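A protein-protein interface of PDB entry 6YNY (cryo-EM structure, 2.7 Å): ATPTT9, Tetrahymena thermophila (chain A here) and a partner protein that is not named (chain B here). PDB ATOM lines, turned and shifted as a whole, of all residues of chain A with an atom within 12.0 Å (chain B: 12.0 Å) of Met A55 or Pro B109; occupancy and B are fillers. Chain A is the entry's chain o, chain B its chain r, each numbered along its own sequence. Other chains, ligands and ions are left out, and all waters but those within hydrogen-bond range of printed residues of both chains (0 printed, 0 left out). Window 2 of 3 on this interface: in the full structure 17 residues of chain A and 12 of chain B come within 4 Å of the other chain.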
ATOM      1  N   MET A  55     -21.012  -2.923 -11.572  1.00  0.00           N
ATOM      2  CA  MET A  55     -19.721  -3.590 -11.460  1.00  0.00           C
ATOM      3  C   MET A  55     -19.122  -3.846 -12.843  1.00  0.00           C
ATOM      4  O   MET A  55     -19.850  -4.115 -13.797  1.00  0.00           O
ATOM      5  CB  MET A  55     -19.872  -4.896 -10.687  1.00  0.00           C
ATOM      6  CG  MET A  55     -18.571  -5.602 -10.412  1.00  0.00           C
ATOM      7  SD  MET A  55     -18.682  -6.715  -9.002  1.00  0.00           S
ATOM      8  CE  MET A  55     -16.954  -7.079  -8.746  1.00  0.00           C
ATOM      9  N   GLN A  56     -17.796  -3.763 -12.944  1.00  0.00           N
ATOM     10  CA  GLN A  56     -17.124  -3.893 -14.230  1.00  0.00           C
ATOM     11  C   GLN A  56     -17.558  -5.163 -14.946  1.00  0.00           C
ATOM     12  O   GLN A  56     -17.594  -6.245 -14.357  1.00  0.00           O
ATOM     13  CB  GLN A  56     -15.607  -3.897 -14.046  1.00  0.00           C
ATOM     14  CG  GLN A  56     -14.982  -2.540 -13.837  1.00  0.00           C
ATOM     15  CD  GLN A  56     -14.934  -2.131 -12.383  1.00  0.00           C
ATOM     16  OE1 GLN A  56     -15.817  -2.469 -11.597  1.00  0.00           O
ATOM     17  NE2 GLN A  56     -13.889  -1.408 -12.013  1.00  0.00           N
ATOM     18  N   ASN A  57     -17.880  -5.020 -16.232  1.00  0.00           N
ATOM     19  CA  ASN A  57     -18.374  -6.155 -17.003  1.00  0.00           C
ATOM     20  C   ASN A  57     -17.279  -7.186 -17.233  1.00  0.00           C
ATOM     21  O   ASN A  57     -17.543  -8.393 -17.221  1.00  0.00           O
ATOM     22  CB  ASN A  57     -18.943  -5.666 -18.334  1.00  0.00           C
ATOM     23  CG  ASN A  57     -17.975  -4.781 -19.092  1.00  0.00           C
ATOM     24  OD1 ASN A  57     -16.795  -4.703 -18.757  1.00  0.00           O
ATOM     25  ND2 ASN A  57     -18.470  -4.105 -20.117  1.00  0.00           N
ATOM     26  N   THR A  58     -16.048  -6.732 -17.451  1.00  0.00           N
ATOM     27  CA  THR A  58     -14.927  -7.630 -17.712  1.00  0.00           C
ATOM     28  C   THR A  58     -14.183  -7.930 -16.411  1.00  0.00           C
ATOM     29  O   THR A  58     -12.982  -7.708 -16.275  1.00  0.00           O
ATOM     30  CB  THR A  58     -13.994  -7.025 -18.752  1.00  0.00           C
ATOM     31  OG1 THR A  58     -13.557  -5.736 -18.309  1.00  0.00           O
ATOM     32  CG2 THR A  58     -14.684  -6.893 -20.088  1.00  0.00           C
ATOM     33  N   THR A  59     -14.930  -8.451 -15.446  1.00  0.00           N
ATOM     34  CA  THR A  59     -14.398  -8.817 -14.142  1.00  0.00           C
ATOM     35  C   THR A  59     -14.444 -10.326 -13.978  1.00  0.00           C
ATOM     36  O   THR A  59     -15.497 -10.945 -14.165  1.00  0.00           O
ATOM     37  CB  THR A  59     -15.181  -8.150 -13.015  1.00  0.00           C
ATOM     38  OG1 THR A  59     -15.091  -6.729 -13.143  1.00  0.00           O
ATOM     39  CG2 THR A  59     -14.628  -8.564 -11.676  1.00  0.00           C
ATOM     40  N   ASN A  60     -13.306 -10.908 -13.623  1.00  0.00           N
ATOM     41  CA  ASN A  60     -13.187 -12.341 -13.430  1.00  0.00           C
ATOM     42  C   ASN A  60     -12.395 -12.603 -12.160  1.00  0.00           C
ATOM     43  O   ASN A  60     -11.464 -11.863 -11.838  1.00  0.00           O
ATOM     44  CB  ASN A  60     -12.500 -13.016 -14.622  1.00  0.00           C
ATOM     45  CG  ASN A  60     -13.241 -12.808 -15.918  1.00  0.00           C
ATOM     46  OD1 ASN A  60     -12.651 -12.427 -16.926  1.00  0.00           O
ATOM     47  ND2 ASN A  60     -14.542 -13.054 -15.902  1.00  0.00           N
ATOM     48  N   ILE A  61     -12.777 -13.654 -11.444  1.00  0.00           N
ATOM     49  CA  ILE A  61     -12.071 -14.099 -10.251  1.00  0.00           C
ATOM     50  C   ILE A  61     -11.383 -15.409 -10.595  1.00  0.00           C
ATOM     51  O   ILE A  61     -12.045 -16.388 -10.958  1.00  0.00           O
ATOM     52  CB  ILE A  61     -13.019 -14.281  -9.056  1.00  0.00           C
ATOM     53  CG1 ILE A  61     -13.836 -13.015  -8.796  1.00  0.00           C
ATOM     54  CG2 ILE A  61     -12.233 -14.631  -7.824  1.00  0.00           C
ATOM     55  CD1 ILE A  61     -13.062 -11.894  -8.217  1.00  0.00           C
ATOM     56  N   VAL A  62     -10.060 -15.428 -10.489  1.00  0.00           N
ATOM     57  CA  VAL A  62      -9.255 -16.598 -10.809  1.00  0.00           C
ATOM     58  C   VAL A  62      -8.678 -17.156  -9.519  1.00  0.00           C
ATOM     59  O   VAL A  62      -8.303 -16.401  -8.617  1.00  0.00           O
ATOM     60  CB  VAL A  62      -8.136 -16.264 -11.811  1.00  0.00           C
ATOM     61  CG1 VAL A  62      -7.401 -17.516 -12.208  1.00  0.00           C
ATOM     62  CG2 VAL A  62      -8.712 -15.594 -13.039  1.00  0.00           C
ATOM     63  N   HIS A  63      -8.614 -18.483  -9.433  1.00  0.00           N
ATOM     64  CA  HIS A  63      -8.176 -19.153  -8.220  1.00  0.00           C
ATOM     65  C   HIS A  63      -6.740 -19.645  -8.292  1.00  0.00           C
ATOM     66  O   HIS A  63      -6.185 -20.027  -7.257  1.00  0.00           O
ATOM     67  CB  HIS A  63      -9.100 -20.331  -7.915  1.00  0.00           C
ATOM     68  CG  HIS A  63     -10.447 -19.926  -7.407  1.00  0.00           C
ATOM     69  ND1 HIS A  63     -10.626 -18.884  -6.526  1.00  0.00           N
ATOM     70  CD2 HIS A  63     -11.682 -20.418  -7.665  1.00  0.00           C
ATOM     71  CE1 HIS A  63     -11.913 -18.754  -6.257  1.00  0.00           C
ATOM     72  NE2 HIS A  63     -12.575 -19.673  -6.936  1.00  0.00           N
ATOM     73  N   ARG B 103      -9.291 -21.537 -16.575  1.00  0.00           N
ATOM     74  CA  ARG B 103     -10.641 -21.102 -16.912  1.00  0.00           C
ATOM     75  C   ARG B 103     -11.691 -21.958 -16.225  1.00  0.00           C
ATOM     76  O   ARG B 103     -12.792 -21.474 -15.945  1.00  0.00           O
ATOM     77  CB  ARG B 103     -10.842 -21.118 -18.425  1.00  0.00           C
ATOM     78  CG  ARG B 103     -10.079 -20.044 -19.173  1.00  0.00           C
ATOM     79  CD  ARG B 103     -10.349 -18.666 -18.611  1.00  0.00           C
ATOM     80  NE  ARG B 103      -9.848 -17.594 -19.459  1.00  0.00           N
ATOM     81  CZ  ARG B 103      -9.593 -16.365 -19.026  1.00  0.00           C
ATOM     82  NH1 ARG B 103      -9.779 -16.052 -17.755  1.00  0.00           N
ATOM     83  NH2 ARG B 103      -9.141 -15.445 -19.861  1.00  0.00           N
ATOM     84  N   TYR B 104     -11.383 -23.225 -15.951  1.00  0.00           N
ATOM     85  CA  TYR B 104     -12.278 -24.019 -15.124  1.00  0.00           C
ATOM     86  C   TYR B 104     -12.388 -23.426 -13.728  1.00  0.00           C
ATOM     87  O   TYR B 104     -13.449 -23.502 -13.100  1.00  0.00           O
ATOM     88  CB  TYR B 104     -11.787 -25.463 -15.056  1.00  0.00           C
ATOM     89  CG  TYR B 104     -12.749 -26.403 -14.382  1.00  0.00           C
ATOM     90  CD1 TYR B 104     -13.609 -27.190 -15.124  1.00  0.00           C
ATOM     91  CD2 TYR B 104     -12.804 -26.500 -13.004  1.00  0.00           C
ATOM     92  CE1 TYR B 104     -14.489 -28.046 -14.518  1.00  0.00           C
ATOM     93  CE2 TYR B 104     -13.682 -27.352 -12.389  1.00  0.00           C
ATOM     94  CZ  TYR B 104     -14.523 -28.123 -13.148  1.00  0.00           C
ATOM     95  OH  TYR B 104     -15.400 -28.977 -12.531  1.00  0.00           O
ATOM     96  N   LEU B 105     -11.305 -22.829 -13.235  1.00  0.00           N
ATOM     97  CA  LEU B 105     -11.260 -22.196 -11.928  1.00  0.00           C
ATOM     98  C   LEU B 105     -11.467 -20.692 -12.005  1.00  0.00           C
ATOM     99  O   LEU B 105     -11.143 -19.976 -11.053  1.00  0.00           O
ATOM    100  CB  LEU B 105      -9.927 -22.504 -11.256  1.00  0.00           C
ATOM    101  CG  LEU B 105      -9.662 -23.980 -10.993  1.00  0.00           C
ATOM    102  CD1 LEU B 105      -8.227 -24.191 -10.617  1.00  0.00           C
ATOM    103  CD2 LEU B 105     -10.566 -24.466  -9.900  1.00  0.00           C
ATOM    104  N   THR B 106     -11.994 -20.201 -13.117  1.00  0.00           N
ATOM    105  CA  THR B 106     -12.299 -18.787 -13.293  1.00  0.00           C
ATOM    106  C   THR B 106     -13.800 -18.618 -13.117  1.00  0.00           C
ATOM    107  O   THR B 106     -14.583 -18.963 -14.004  1.00  0.00           O
ATOM    108  CB  THR B 106     -11.840 -18.286 -14.657  1.00  0.00           C
ATOM    109  OG1 THR B 106     -10.410 -18.326 -14.729  1.00  0.00           O
ATOM    110  CG2 THR B 106     -12.314 -16.869 -14.887  1.00  0.00           C
ATOM    111  N   GLU B 107     -14.198 -18.093 -11.968  1.00  0.00           N
ATOM    112  CA  GLU B 107     -15.598 -17.859 -11.672  1.00  0.00           C
ATOM    113  C   GLU B 107     -15.883 -16.365 -11.698  1.00  0.00           C
ATOM    114  O   GLU B 107     -14.976 -15.530 -11.686  1.00  0.00           O
ATOM    115  CB  GLU B 107     -15.975 -18.445 -10.311  1.00  0.00           C
ATOM    116  CG  GLU B 107     -15.263 -17.818  -9.140  1.00  0.00           C
ATOM    117  CD  GLU B 107     -15.737 -18.376  -7.814  1.00  0.00           C
ATOM    118  OE1 GLU B 107     -16.297 -19.491  -7.804  1.00  0.00           O
ATOM    119  OE2 GLU B 107     -15.562 -17.697  -6.780  1.00  0.00           O
ATOM    120  N   ASP B 108     -17.149 -16.047 -11.732  1.00  0.00           N
ATOM    121  CA  ASP B 108     -17.584 -14.669 -11.669  1.00  0.00           C
ATOM    122  C   ASP B 108     -18.109 -14.351 -10.283  1.00  0.00           C
ATOM    123  O   ASP B 108     -18.530 -15.244  -9.545  1.00  0.00           O
ATOM    124  CB  ASP B 108     -18.674 -14.397 -12.710  1.00  0.00           C
ATOM    125  CG  ASP B 108     -19.787 -15.415 -12.665  1.00  0.00           C
ATOM    126  OD1 ASP B 108     -20.594 -15.369 -11.715  1.00  0.00           O
ATOM    127  OD2 ASP B 108     -19.852 -16.263 -13.580  1.00  0.00           O
ATOM    128  N   PRO B 109     -18.081 -13.087  -9.888  1.00  0.00           N
ATOM    129  CA  PRO B 109     -18.471 -12.738  -8.523  1.00  0.00           C
ATOM    130  C   PRO B 109     -19.978 -12.690  -8.348  1.00  0.00           C
ATOM    131  O   PRO B 109     -20.740 -12.470  -9.292  1.00  0.00           O
ATOM    132  CB  PRO B 109     -17.848 -11.353  -8.331  1.00  0.00           C
ATOM    133  CG  PRO B 109     -17.786 -10.784  -9.695  1.00  0.00           C
ATOM    134  CD  PRO B 109     -17.578 -11.922 -10.635  1.00  0.00           C
ATOM    135  N   ALA B 110     -20.402 -12.904  -7.106  1.00  0.00           N
ATOM    136  CA  ALA B 110     -21.747 -12.676  -6.599  1.00  0.00           C
ATOM    137  C   ALA B 110     -22.739 -13.760  -7.009  1.00  0.00           C
ATOM    138  O   ALA B 110     -23.856 -13.773  -6.490  1.00  0.00           O
ATOM    139  CB  ALA B 110     -22.318 -11.316  -7.033  1.00  0.00           C
ATOM    140  N   GLY B 111     -22.381 -14.672  -7.902  1.00  0.00           N
ATOM    141  CA  GLY B 111     -23.306 -15.727  -8.278  1.00  0.00           C
ATOM    142  C   GLY B 111     -24.598 -15.177  -8.841  1.00  0.00           C
ATOM    143  O   GLY B 111     -24.613 -14.184  -9.577  1.00  0.00           O
ATOM    144  N   ASP B 112     -25.706 -15.825  -8.494  1.00  0.00           N
ATOM    145  CA  ASP B 112     -27.020 -15.455  -8.996  1.00  0.00           C
ATOM    146  C   ASP B 112     -27.840 -14.753  -7.922  1.00  0.00           C
ATOM    147  O   ASP B 112     -27.478 -14.707  -6.745  1.00  0.00           O
ATOM    148  CB  ASP B 112     -27.773 -16.685  -9.511  1.00  0.00           C
ATOM    149  CG  ASP B 112     -27.326 -17.108 -10.897  1.00  0.00           C
ATOM    150  OD1 ASP B 112     -26.865 -16.239 -11.666  1.00  0.00           O
ATOM    151  OD2 ASP B 112     -27.442 -18.307 -11.221  1.00  0.00           O
ATOM    152  N   ASP B 113     -28.972 -14.219  -8.360  1.00  0.00           N
ATOM    153  CA  ASP B 113     -29.844 -13.428  -7.509  1.00  0.00           C
ATOM    154  C   ASP B 113     -30.380 -14.276  -6.363  1.00  0.00           C
ATOM    155  O   ASP B 113     -31.092 -15.259  -6.614  1.00  0.00           O
ATOM    156  CB  ASP B 113     -30.997 -12.865  -8.332  1.00  0.00           C
ATOM    157  CG  ASP B 113     -31.712 -11.729  -7.636  1.00  0.00           C
ATOM    158  OD1 ASP B 113     -31.314 -11.366  -6.510  1.00  0.00           O
ATOM    159  OD2 ASP B 113     -32.674 -11.190  -8.219  1.00  0.00           O
ATOM    160  N   PRO B 114     -30.073 -13.947  -5.108  1.00  0.00           N
ATOM    161  CA  PRO B 114     -30.668 -14.699  -3.994  1.00  0.00           C
ATOM    162  C   PRO B 114     -32.173 -14.555  -3.907  1.00  0.00           C
ATOM    163  O   PRO B 114     -32.832 -15.421  -3.319  1.00  0.00           O
ATOM    164  CB  PRO B 114     -29.982 -14.102  -2.759  1.00  0.00           C
ATOM    165  CG  PRO B 114     -28.755 -13.451  -3.270  1.00  0.00           C
ATOM    166  CD  PRO B 114     -29.088 -12.964  -4.635  1.00  0.00           C
ATOM    167  N   LYS B 117     -34.360 -17.358  -5.112  1.00  0.00           N
ATOM    168  CA  LYS B 117     -34.171 -18.597  -4.382  1.00  0.00           C
ATOM    169  C   LYS B 117     -35.158 -18.694  -3.227  1.00  0.00           C
ATOM    170  O   LYS B 117     -35.740 -17.699  -2.788  1.00  0.00           O
ATOM    171  CB  LYS B 117     -32.738 -18.695  -3.859  1.00  0.00           C
ATOM    172  CG  LYS B 117     -31.710 -18.803  -4.958  1.00  0.00           C
ATOM    173  CD  LYS B 117     -30.304 -18.880  -4.419  1.00  0.00           C
ATOM    174  CE  LYS B 117     -29.311 -19.088  -5.545  1.00  0.00           C
ATOM    175  NZ  LYS B 117     -27.925 -19.243  -5.048  1.00  0.00           N
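The backbone NH (N) of Ile A61 lies within hydrogen-bond range of the backbone carbonyl oxygen (O) of Glu B107.
The backbone carbonyl oxygen (O) of Leu B105 lies within hydrogen-bond range of the backbone NH (N) of His A63.
Among the printed residues, merely in contact across the chains: Ile A61 with Thr B106 (3.4 Å), His A63 with Glu B107 (3.5 Å), Val A62 with Thr B106 (3.6 Å), Ile A61 with Leu B105 (3.7 Å), Asn A60 with Thr B106 (3.9 Å), Val A62 with Leu B105 (3.9 Å), Met A55 with Pro B109 (3.9 Å) and Asn A60 with Glu B107 (3.9 Å).
Met A55 touches just one residue of chain B: Pro B109.
Of chain A, only Met A55 (3.9 Å) comes within 4 Å of Pro B109.
No residue of chain B comes within 4 Å of Gln A56.
No residue of chain B comes within 4 Å of Asn A57.
Of chain B, only Leu B105 (3.7 Å), Thr B106 (3.4 Å) and Glu B107 (2.9 Å) come within 4 Å of Ile A61.
Of chain A, only Asn A60 (3.9 Å), Ile A61 (2.9 Å) and His A63 (3.5 Å) come within 4 Å of Glu B107.
No residue of chain A comes within 4 Å of Asp B108.
No residue of chain A comes within 4 Å of Ala B110.
No residue of chain A comes within 4 Å of Gly B111.
Of the printed residues of chain A, Leu B105 touches Ile A61, Val A62 and His A63.
Of the printed residues of chain B, Val A62 touches Leu B105 (3.9 Å) and Thr B106 (3.6 Å).
Of the printed residues of chain B, His A63 touches Leu B105 and Glu B107.
Of the printed residues of chain B, Asn A60 touches Thr B106 and Glu B107.
Of the printed residues of chain A, Thr B106 touches Asn A60 (3.9 Å), Ile A61 (3.4 Å) and Val A62 (3.6 Å).
The nearest residue of chain B that does not touch Met A55 is Ala B110 (6.2 Å).
The nearest printed residue of chain B that does not touch Val A62 is Arg B103 (4.9 Å).
Of the 13 printed residues of chain B, 4 touch a printed residue of chain A.
Of the 9 printed residues of chain A, 5 touch a printed residue of chain B.
Hydrophobic or aromatic side chains of chain A within 4 Å of the printed part of chain B: Met A55, Ile A61, Val A62 and His A63.
Among the printed residues, 10 pairs touch across the chains.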
